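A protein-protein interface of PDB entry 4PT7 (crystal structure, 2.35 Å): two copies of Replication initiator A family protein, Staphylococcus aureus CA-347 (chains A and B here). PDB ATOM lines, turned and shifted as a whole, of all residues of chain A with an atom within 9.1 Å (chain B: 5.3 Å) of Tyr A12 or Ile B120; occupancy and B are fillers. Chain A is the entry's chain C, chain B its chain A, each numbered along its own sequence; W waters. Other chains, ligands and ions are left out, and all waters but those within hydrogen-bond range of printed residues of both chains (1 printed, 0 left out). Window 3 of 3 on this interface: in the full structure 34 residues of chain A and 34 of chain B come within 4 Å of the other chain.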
ATOM      1  N   PHE A   6      -1.518   8.329 -16.112  1.00  0.00           N
ATOM      2  CA  PHE A   6      -2.206   7.652 -17.192  1.00  0.00           C
ATOM      3  C   PHE A   6      -2.671   6.368 -16.521  1.00  0.00           C
ATOM      4  O   PHE A   6      -1.848   5.554 -16.109  1.00  0.00           O
ATOM      5  CB  PHE A   6      -1.251   7.309 -18.346  1.00  0.00           C
ATOM      6  CG  PHE A   6      -0.926   8.476 -19.244  1.00  0.00           C
ATOM      7  CD1 PHE A   6       0.205   9.258 -19.024  1.00  0.00           C
ATOM      8  CD2 PHE A   6      -1.753   8.787 -20.319  1.00  0.00           C
ATOM      9  CE1 PHE A   6       0.506  10.331 -19.857  1.00  0.00           C
ATOM     10  CE2 PHE A   6      -1.464   9.860 -21.163  1.00  0.00           C
ATOM     11  CZ  PHE A   6      -0.329  10.636 -20.932  1.00  0.00           C
ATOM     12  N   THR A   7      -3.982   6.191 -16.399  1.00  0.00           N
ATOM     13  CA  THR A   7      -4.528   4.996 -15.761  1.00  0.00           C
ATOM     14  C   THR A   7      -4.987   3.974 -16.790  1.00  0.00           C
ATOM     15  O   THR A   7      -5.267   4.325 -17.931  1.00  0.00           O
ATOM     16  CB  THR A   7      -5.729   5.341 -14.858  1.00  0.00           C
ATOM     17  OG1 THR A   7      -6.830   5.772 -15.668  1.00  0.00           O
ATOM     18  CG2 THR A   7      -5.361   6.470 -13.886  1.00  0.00           C
ATOM     19  N   VAL A   8      -5.052   2.709 -16.394  1.00  0.00           N
ATOM     20  CA  VAL A   8      -5.500   1.667 -17.312  1.00  0.00           C
ATOM     21  C   VAL A   8      -6.999   1.790 -17.568  1.00  0.00           C
ATOM     22  O   VAL A   8      -7.471   1.482 -18.663  1.00  0.00           O
ATOM     23  CB  VAL A   8      -5.199   0.251 -16.773  1.00  0.00           C
ATOM     24  CG1 VAL A   8      -3.715  -0.040 -16.885  1.00  0.00           C
ATOM     25  CG2 VAL A   8      -5.649   0.138 -15.322  1.00  0.00           C
ATOM     26  N   GLN A   9      -7.741   2.246 -16.559  1.00  0.00           N
ATOM     27  CA  GLN A   9      -9.188   2.419 -16.688  1.00  0.00           C
ATOM     28  C   GLN A   9      -9.488   3.363 -17.852  1.00  0.00           C
ATOM     29  O   GLN A   9     -10.234   3.027 -18.771  1.00  0.00           O
ATOM     30  CB  GLN A   9      -9.783   3.025 -15.413  1.00  0.00           C
ATOM     31  CG  GLN A   9      -9.675   2.176 -14.141  1.00  0.00           C
ATOM     32  CD  GLN A   9      -8.252   2.078 -13.599  1.00  0.00           C
ATOM     33  OE1 GLN A   9      -7.543   3.112 -13.559  1.00  0.00           O
ATOM     34  NE2 GLN A   9      -7.850   0.962 -13.201  1.00  0.00           N
ATOM     35  N   GLU A  10      -8.891   4.547 -17.800  1.00  0.00           N
ATOM     36  CA  GLU A  10      -9.084   5.554 -18.832  1.00  0.00           C
ATOM     37  C   GLU A  10      -8.623   5.010 -20.179  1.00  0.00           C
ATOM     38  O   GLU A  10      -9.301   5.186 -21.188  1.00  0.00           O
ATOM     39  CB  GLU A  10      -8.311   6.830 -18.459  1.00  0.00           C
ATOM     40  CG  GLU A  10      -8.751   8.098 -19.183  1.00  0.00           C
ATOM     41  CD  GLU A  10     -10.232   8.432 -18.949  1.00  0.00           C
ATOM     42  OE1 GLU A  10     -10.709   8.326 -17.785  1.00  0.00           O
ATOM     43  OE2 GLU A  10     -10.913   8.808 -19.933  1.00  0.00           O
ATOM     44  N   ASN A  11      -7.489   4.319 -20.194  1.00  0.00           N
ATOM     45  CA  ASN A  11      -6.991   3.776 -21.441  1.00  0.00           C
ATOM     46  C   ASN A  11      -7.978   2.811 -22.106  1.00  0.00           C
ATOM     47  O   ASN A  11      -8.248   2.921 -23.303  1.00  0.00           O
ATOM     48  CB  ASN A  11      -5.661   3.077 -21.221  1.00  0.00           C
ATOM     49  CG  ASN A  11      -5.008   2.684 -22.526  1.00  0.00           C
ATOM     50  OD1 ASN A  11      -5.469   1.774 -23.212  1.00  0.00           O
ATOM     51  ND2 ASN A  11      -3.946   3.389 -22.893  1.00  0.00           N
ATOM     52  N   TYR A  12      -8.517   1.869 -21.338  1.00  0.00           N
ATOM     53  CA  TYR A  12      -9.468   0.900 -21.885  1.00  0.00           C
ATOM     54  C   TYR A  12     -10.827   1.553 -22.118  1.00  0.00           C
ATOM     55  O   TYR A  12     -11.616   1.120 -22.942  1.00  0.00           O
ATOM     56  CB  TYR A  12      -9.584  -0.304 -20.942  1.00  0.00           C
ATOM     57  CG  TYR A  12      -8.467  -1.311 -21.137  1.00  0.00           C
ATOM     58  CD1 TYR A  12      -8.502  -2.218 -22.195  1.00  0.00           C
ATOM     59  CD2 TYR A  12      -7.362  -1.336 -20.287  1.00  0.00           C
ATOM     60  CE1 TYR A  12      -7.466  -3.132 -22.405  1.00  0.00           C
ATOM     61  CE2 TYR A  12      -6.315  -2.249 -20.487  1.00  0.00           C
ATOM     62  CZ  TYR A  12      -6.377  -3.144 -21.548  1.00  0.00           C
ATOM     63  OH  TYR A  12      -5.364  -4.062 -21.744  1.00  0.00           O
ATOM     64  N   LYS A  13     -11.070   2.634 -21.400  1.00  0.00           N
ATOM     65  CA  LYS A  13     -12.302   3.386 -21.526  1.00  0.00           C
ATOM     66  C   LYS A  13     -12.261   4.163 -22.846  1.00  0.00           C
ATOM     67  O   LYS A  13     -13.304   4.437 -23.447  1.00  0.00           O
ATOM     68  CB  LYS A  13     -12.410   4.350 -20.345  1.00  0.00           C
ATOM     69  CG  LYS A  13     -13.779   4.888 -20.067  1.00  0.00           C
ATOM     70  CD  LYS A  13     -13.756   5.684 -18.752  1.00  0.00           C
ATOM     71  CE  LYS A  13     -13.370   4.813 -17.560  1.00  0.00           C
ATOM     72  NZ  LYS A  13     -13.467   5.534 -16.249  1.00  0.00           N
ATOM     73  N   GLU A  14     -11.056   4.501 -23.301  1.00  0.00           N
ATOM     74  CA  GLU A  14     -10.910   5.253 -24.537  1.00  0.00           C
ATOM     75  C   GLU A  14     -10.622   4.394 -25.768  1.00  0.00           C
ATOM     76  O   GLU A  14      -9.878   4.796 -26.655  1.00  0.00           O
ATOM     77  CB  GLU A  14      -9.832   6.329 -24.376  1.00  0.00           C
ATOM     78  CG  GLU A  14     -10.216   7.460 -23.418  1.00  0.00           C
ATOM     79  CD  GLU A  14     -11.357   8.333 -23.940  1.00  0.00           C
ATOM     80  OE1 GLU A  14     -12.364   8.496 -23.215  1.00  0.00           O
ATOM     81  OE2 GLU A  14     -11.243   8.862 -25.069  1.00  0.00           O
ATOM     82  N   ARG A  15     -11.221   3.211 -25.811  1.00  0.00           N
ATOM     83  CA  ARG A  15     -11.080   2.316 -26.958  1.00  0.00           C
ATOM     84  C   ARG A  15     -12.473   2.178 -27.566  1.00  0.00           C
ATOM     85  O   ARG A  15     -13.455   1.943 -26.845  1.00  0.00           O
ATOM     86  CB  ARG A  15     -10.523   0.959 -26.508  1.00  0.00           C
ATOM     87  CG  ARG A  15      -9.152   1.116 -25.852  1.00  0.00           C
ATOM     88  CD  ARG A  15      -8.414  -0.188 -25.687  1.00  0.00           C
ATOM     89  NE  ARG A  15      -7.135   0.013 -25.011  1.00  0.00           N
ATOM     90  CZ  ARG A  15      -6.195  -0.919 -24.917  1.00  0.00           C
ATOM     91  NH1 ARG A  15      -6.399  -2.110 -25.459  1.00  0.00           N
ATOM     92  NH2 ARG A  15      -5.060  -0.668 -24.278  1.00  0.00           N
ATOM     93  N   PHE A  16     -12.572   2.338 -28.881  1.00  0.00           N
ATOM     94  CA  PHE A  16     -13.876   2.268 -29.523  1.00  0.00           C
ATOM     95  C   PHE A  16     -13.884   1.564 -30.872  1.00  0.00           C
ATOM     96  O   PHE A  16     -12.843   1.202 -31.419  1.00  0.00           O
ATOM     97  CB  PHE A  16     -14.462   3.685 -29.749  1.00  0.00           C
ATOM     98  CG  PHE A  16     -13.986   4.736 -28.768  1.00  0.00           C
ATOM     99  CD1 PHE A  16     -12.689   5.231 -28.839  1.00  0.00           C
ATOM    100  CD2 PHE A  16     -14.843   5.250 -27.790  1.00  0.00           C
ATOM    101  CE1 PHE A  16     -12.242   6.224 -27.953  1.00  0.00           C
ATOM    102  CE2 PHE A  16     -14.407   6.244 -26.896  1.00  0.00           C
ATOM    103  CZ  PHE A  16     -13.100   6.731 -26.982  1.00  0.00           C
ATOM    104  N   VAL B 115     -15.138   0.643 -16.390  1.00  0.00           N
ATOM    105  CA  VAL B 115     -14.369  -0.505 -16.845  1.00  0.00           C
ATOM    106  C   VAL B 115     -13.968  -1.364 -15.664  1.00  0.00           C
ATOM    107  O   VAL B 115     -13.421  -0.860 -14.681  1.00  0.00           O
ATOM    108  CB  VAL B 115     -13.089  -0.056 -17.591  1.00  0.00           C
ATOM    109  CG1 VAL B 115     -12.196  -1.243 -17.855  1.00  0.00           C
ATOM    110  CG2 VAL B 115     -13.467   0.616 -18.903  1.00  0.00           C
ATOM    111  N   THR B 116     -14.241  -2.660 -15.758  1.00  0.00           N
ATOM    112  CA  THR B 116     -13.883  -3.592 -14.690  1.00  0.00           C
ATOM    113  C   THR B 116     -12.695  -4.426 -15.157  1.00  0.00           C
ATOM    114  O   THR B 116     -12.293  -4.352 -16.324  1.00  0.00           O
ATOM    115  CB  THR B 116     -15.036  -4.563 -14.359  1.00  0.00           C
ATOM    116  OG1 THR B 116     -15.277  -5.416 -15.485  1.00  0.00           O
ATOM    117  CG2 THR B 116     -16.310  -3.798 -14.023  1.00  0.00           C
ATOM    118  N   GLU B 117     -12.144  -5.224 -14.245  1.00  0.00           N
ATOM    119  CA  GLU B 117     -11.014  -6.091 -14.564  1.00  0.00           C
ATOM    120  C   GLU B 117     -11.418  -7.069 -15.665  1.00  0.00           C
ATOM    121  O   GLU B 117     -10.605  -7.447 -16.502  1.00  0.00           O
ATOM    122  CB  GLU B 117     -10.576  -6.868 -13.319  1.00  0.00           C
ATOM    123  CG  GLU B 117      -9.998  -5.997 -12.211  1.00  0.00           C
ATOM    124  CD  GLU B 117      -9.717  -6.782 -10.933  1.00  0.00           C
ATOM    125  OE1 GLU B 117     -10.687  -7.257 -10.296  1.00  0.00           O
ATOM    126  OE2 GLU B 117      -8.527  -6.928 -10.572  1.00  0.00           O
ATOM    127  N   ARG B 118     -12.681  -7.475 -15.662  1.00  0.00           N
ATOM    128  CA  ARG B 118     -13.168  -8.408 -16.668  1.00  0.00           C
ATOM    129  C   ARG B 118     -13.217  -7.741 -18.039  1.00  0.00           C
ATOM    130  O   ARG B 118     -12.892  -8.368 -19.045  1.00  0.00           O
ATOM    131  CB  ARG B 118     -14.562  -8.928 -16.295  1.00  0.00           C
ATOM    132  CG  ARG B 118     -14.628  -9.728 -14.995  1.00  0.00           C
ATOM    133  CD  ARG B 118     -13.858 -11.049 -15.077  1.00  0.00           C
ATOM    134  NE  ARG B 118     -12.419 -10.881 -14.866  1.00  0.00           N
ATOM    135  CZ  ARG B 118     -11.509 -11.827 -15.087  1.00  0.00           C
ATOM    136  NH1 ARG B 118     -11.877 -13.022 -15.535  1.00  0.00           N
ATOM    137  NH2 ARG B 118     -10.224 -11.578 -14.856  1.00  0.00           N
ATOM    138  N   ASP B 119     -13.630  -6.476 -18.074  1.00  0.00           N
ATOM    139  CA  ASP B 119     -13.705  -5.746 -19.336  1.00  0.00           C
ATOM    140  C   ASP B 119     -12.311  -5.648 -19.938  1.00  0.00           C
ATOM    141  O   ASP B 119     -12.115  -5.926 -21.122  1.00  0.00           O
ATOM    142  CB  ASP B 119     -14.274  -4.334 -19.127  1.00  0.00           C
ATOM    143  CG  ASP B 119     -15.743  -4.341 -18.724  1.00  0.00           C
ATOM    144  OD1 ASP B 119     -16.507  -5.164 -19.270  1.00  0.00           O
ATOM    145  OD2 ASP B 119     -16.134  -3.512 -17.874  1.00  0.00           O
ATOM    146  N   ILE B 120     -11.346  -5.254 -19.110  1.00  0.00           N
ATOM    147  CA  ILE B 120      -9.963  -5.120 -19.543  1.00  0.00           C
ATOM    148  C   ILE B 120      -9.469  -6.442 -20.123  1.00  0.00           C
ATOM    149  O   ILE B 120      -8.923  -6.489 -21.228  1.00  0.00           O
ATOM    150  CB  ILE B 120      -9.065  -4.709 -18.362  1.00  0.00           C
ATOM    151  CG1 ILE B 120      -9.455  -3.305 -17.893  1.00  0.00           C
ATOM    152  CG2 ILE B 120      -7.598  -4.765 -18.771  1.00  0.00           C
ATOM    153  CD1 ILE B 120      -8.775  -2.864 -16.613  1.00  0.00           C
ATOM    154  N   TYR B 121      -9.677  -7.518 -19.375  1.00  0.00           N
ATOM    155  CA  TYR B 121      -9.260  -8.840 -19.811  1.00  0.00           C
ATOM    156  C   TYR B 121      -9.888  -9.195 -21.155  1.00  0.00           C
ATOM    157  O   TYR B 121      -9.206  -9.666 -22.061  1.00  0.00           O
ATOM    158  CB  TYR B 121      -9.659  -9.889 -18.773  1.00  0.00           C
ATOM    159  CG  TYR B 121      -9.259 -11.296 -19.149  1.00  0.00           C
ATOM    160  CD1 TYR B 121      -7.941 -11.726 -19.011  1.00  0.00           C
ATOM    161  CD2 TYR B 121     -10.196 -12.195 -19.657  1.00  0.00           C
ATOM    162  CE1 TYR B 121      -7.562 -13.018 -19.366  1.00  0.00           C
ATOM    163  CE2 TYR B 121      -9.830 -13.489 -20.017  1.00  0.00           C
ATOM    164  CZ  TYR B 121      -8.511 -13.895 -19.869  1.00  0.00           C
ATOM    165  OH  TYR B 121      -8.138 -15.175 -20.222  1.00  0.00           O
ATOM    166  N   LYS B 122     -11.191  -8.982 -21.285  1.00  0.00           N
ATOM    167  CA  LYS B 122     -11.862  -9.305 -22.537  1.00  0.00           C
ATOM    168  C   LYS B 122     -11.356  -8.466 -23.701  1.00  0.00           C
ATOM    169  O   LYS B 122     -11.008  -9.003 -24.754  1.00  0.00           O
ATOM    170  CB  LYS B 122     -13.377  -9.129 -22.415  1.00  0.00           C
ATOM    171  CG  LYS B 122     -14.123 -10.308 -21.802  1.00  0.00           C
ATOM    172  CD  LYS B 122     -15.612 -10.209 -22.154  1.00  0.00           C
ATOM    173  CE  LYS B 122     -16.417 -11.420 -21.698  1.00  0.00           C
ATOM    174  NZ  LYS B 122     -16.528 -11.520 -20.216  1.00  0.00           N
ATOM    175  N   ILE B 123     -11.312  -7.152 -23.518  1.00  0.00           N
ATOM    176  CA  ILE B 123     -10.854  -6.282 -24.587  1.00  0.00           C
ATOM    177  C   ILE B 123      -9.435  -6.605 -25.030  1.00  0.00           C
ATOM    178  O   ILE B 123      -9.169  -6.735 -26.222  1.00  0.00           O
ATOM    179  CB  ILE B 123     -10.938  -4.806 -24.176  1.00  0.00           C
ATOM    180  CG1 ILE B 123     -12.406  -4.437 -23.938  1.00  0.00           C
ATOM    181  CG2 ILE B 123     -10.327  -3.923 -25.266  1.00  0.00           C
ATOM    182  CD1 ILE B 123     -12.621  -3.041 -23.420  1.00  0.00           C
ATOM    183  N   GLU B 124      -8.531  -6.744 -24.066  1.00  0.00           N
ATOM    184  CA  GLU B 124      -7.131  -7.038 -24.363  1.00  0.00           C
ATOM    185  C   GLU B 124      -7.001  -8.368 -25.095  1.00  0.00           C
ATOM    186  O   GLU B 124      -6.189  -8.515 -26.009  1.00  0.00           O
ATOM    187  CB  GLU B 124      -6.315  -7.071 -23.066  1.00  0.00           C
ATOM    188  CG  GLU B 124      -4.806  -7.037 -23.255  1.00  0.00           C
ATOM    189  CD  GLU B 124      -4.333  -5.832 -24.073  1.00  0.00           C
ATOM    190  OE1 GLU B 124      -5.002  -4.773 -24.036  1.00  0.00           O
ATOM    191  OE2 GLU B 124      -3.280  -5.941 -24.745  1.00  0.00           O
ATOM    192  N   LYS B 125      -7.811  -9.335 -24.683  1.00  0.00           N
ATOM    193  CA  LYS B 125      -7.803 -10.651 -25.296  1.00  0.00           C
ATOM    194  C   LYS B 125      -8.197 -10.558 -26.770  1.00  0.00           C
ATOM    195  O   LYS B 125      -7.557 -11.168 -27.627  1.00  0.00           O
ATOM    196  CB  LYS B 125      -8.782 -11.574 -24.559  1.00  0.00           C
ATOM    197  CG  LYS B 125      -9.021 -12.916 -25.240  1.00  0.00           C
ATOM    198  CD  LYS B 125     -10.084 -13.725 -24.509  1.00  0.00           C
ATOM    199  CE  LYS B 125     -10.438 -15.010 -25.261  1.00  0.00           C
ATOM    200  NZ  LYS B 125      -9.278 -15.934 -25.405  1.00  0.00           N
HETATM  201  O   HOH W   1     -13.439   2.654 -14.916  1.00  0.00           O
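The side-chain carboxylate (OE1) of Glu B124 is in salt-bridge range of the guanidinium group (NH1) of Arg A15, at 3.3 Å. The side-chain carboxylate (OE1) of Glu B124 sits at hydrogen-bond distance from the side-chain hydroxyl (OH) of Tyr A12, 2.4 Å away.
Water W1 lies within hydrogen-bond range of the backbone NH of Val B115 and the side-chain amino group of Lys A13.
Among the printed residues, pairs that only touch across the chains: Tyr A12 with Ile B120 (3.3 Å), Tyr A12 with Ile B123 (3.96 Å) and Lys A13 with Val B115 (3.99 Å).
No position is printed for both chains. Of the 5 pairs that touch across the chains among the printed residues, none has its exchanged pair printed and touching as well.
OD1 of Asn A11 is in hydrogen-bond range of NH2 of Arg A15 (2.7 Å).
Phe A6 touches none of the printed residues of chain B. Glu A10 touches none of the printed residues of chain B. Of chain B, only Ile B120 (3.3 Å), Ile B123 (3.96 Å) and Glu B124 (2.4 Å) come within 4 Å of Tyr A12. Of the printed residues of chain B, Lys A13 touches Val B115 (3.99 Å). Of the printed residues of chain B, Arg A15 touches Glu B124. Of the printed residues of chain A, Ile B120 touches Tyr A12. Of chain A, only Tyr A12 (3.96 Å) comes within 4 Å of Ile B123. Printed residues of chain A within 4 Å of Glu B124: Tyr A12 and Arg A15. The nearest residue of chain B that does not touch Tyr A12 is Val B115 (4.2 Å). The nearest residue of chain A that does not touch Ile B120 is Val A8 (4.5 Å). The nearest printed residue of chain B that does not touch Arg A15 is Ile B123 (4.2 Å).
Of the 11 printed residues of chain B, 4 touch a printed residue of chain A. Hydrophobic or aromatic side chains of chain A within 4 Å of the printed part of chain B: Tyr A12. Among the printed residues, 5 pairs touch across the chains. Among the printed residues, Asp or Glu carboxylates within 4 Å of a Lys or Arg side-chain nitrogen of the other chain: Arg A15 with Glu B124 (3.3 Å).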
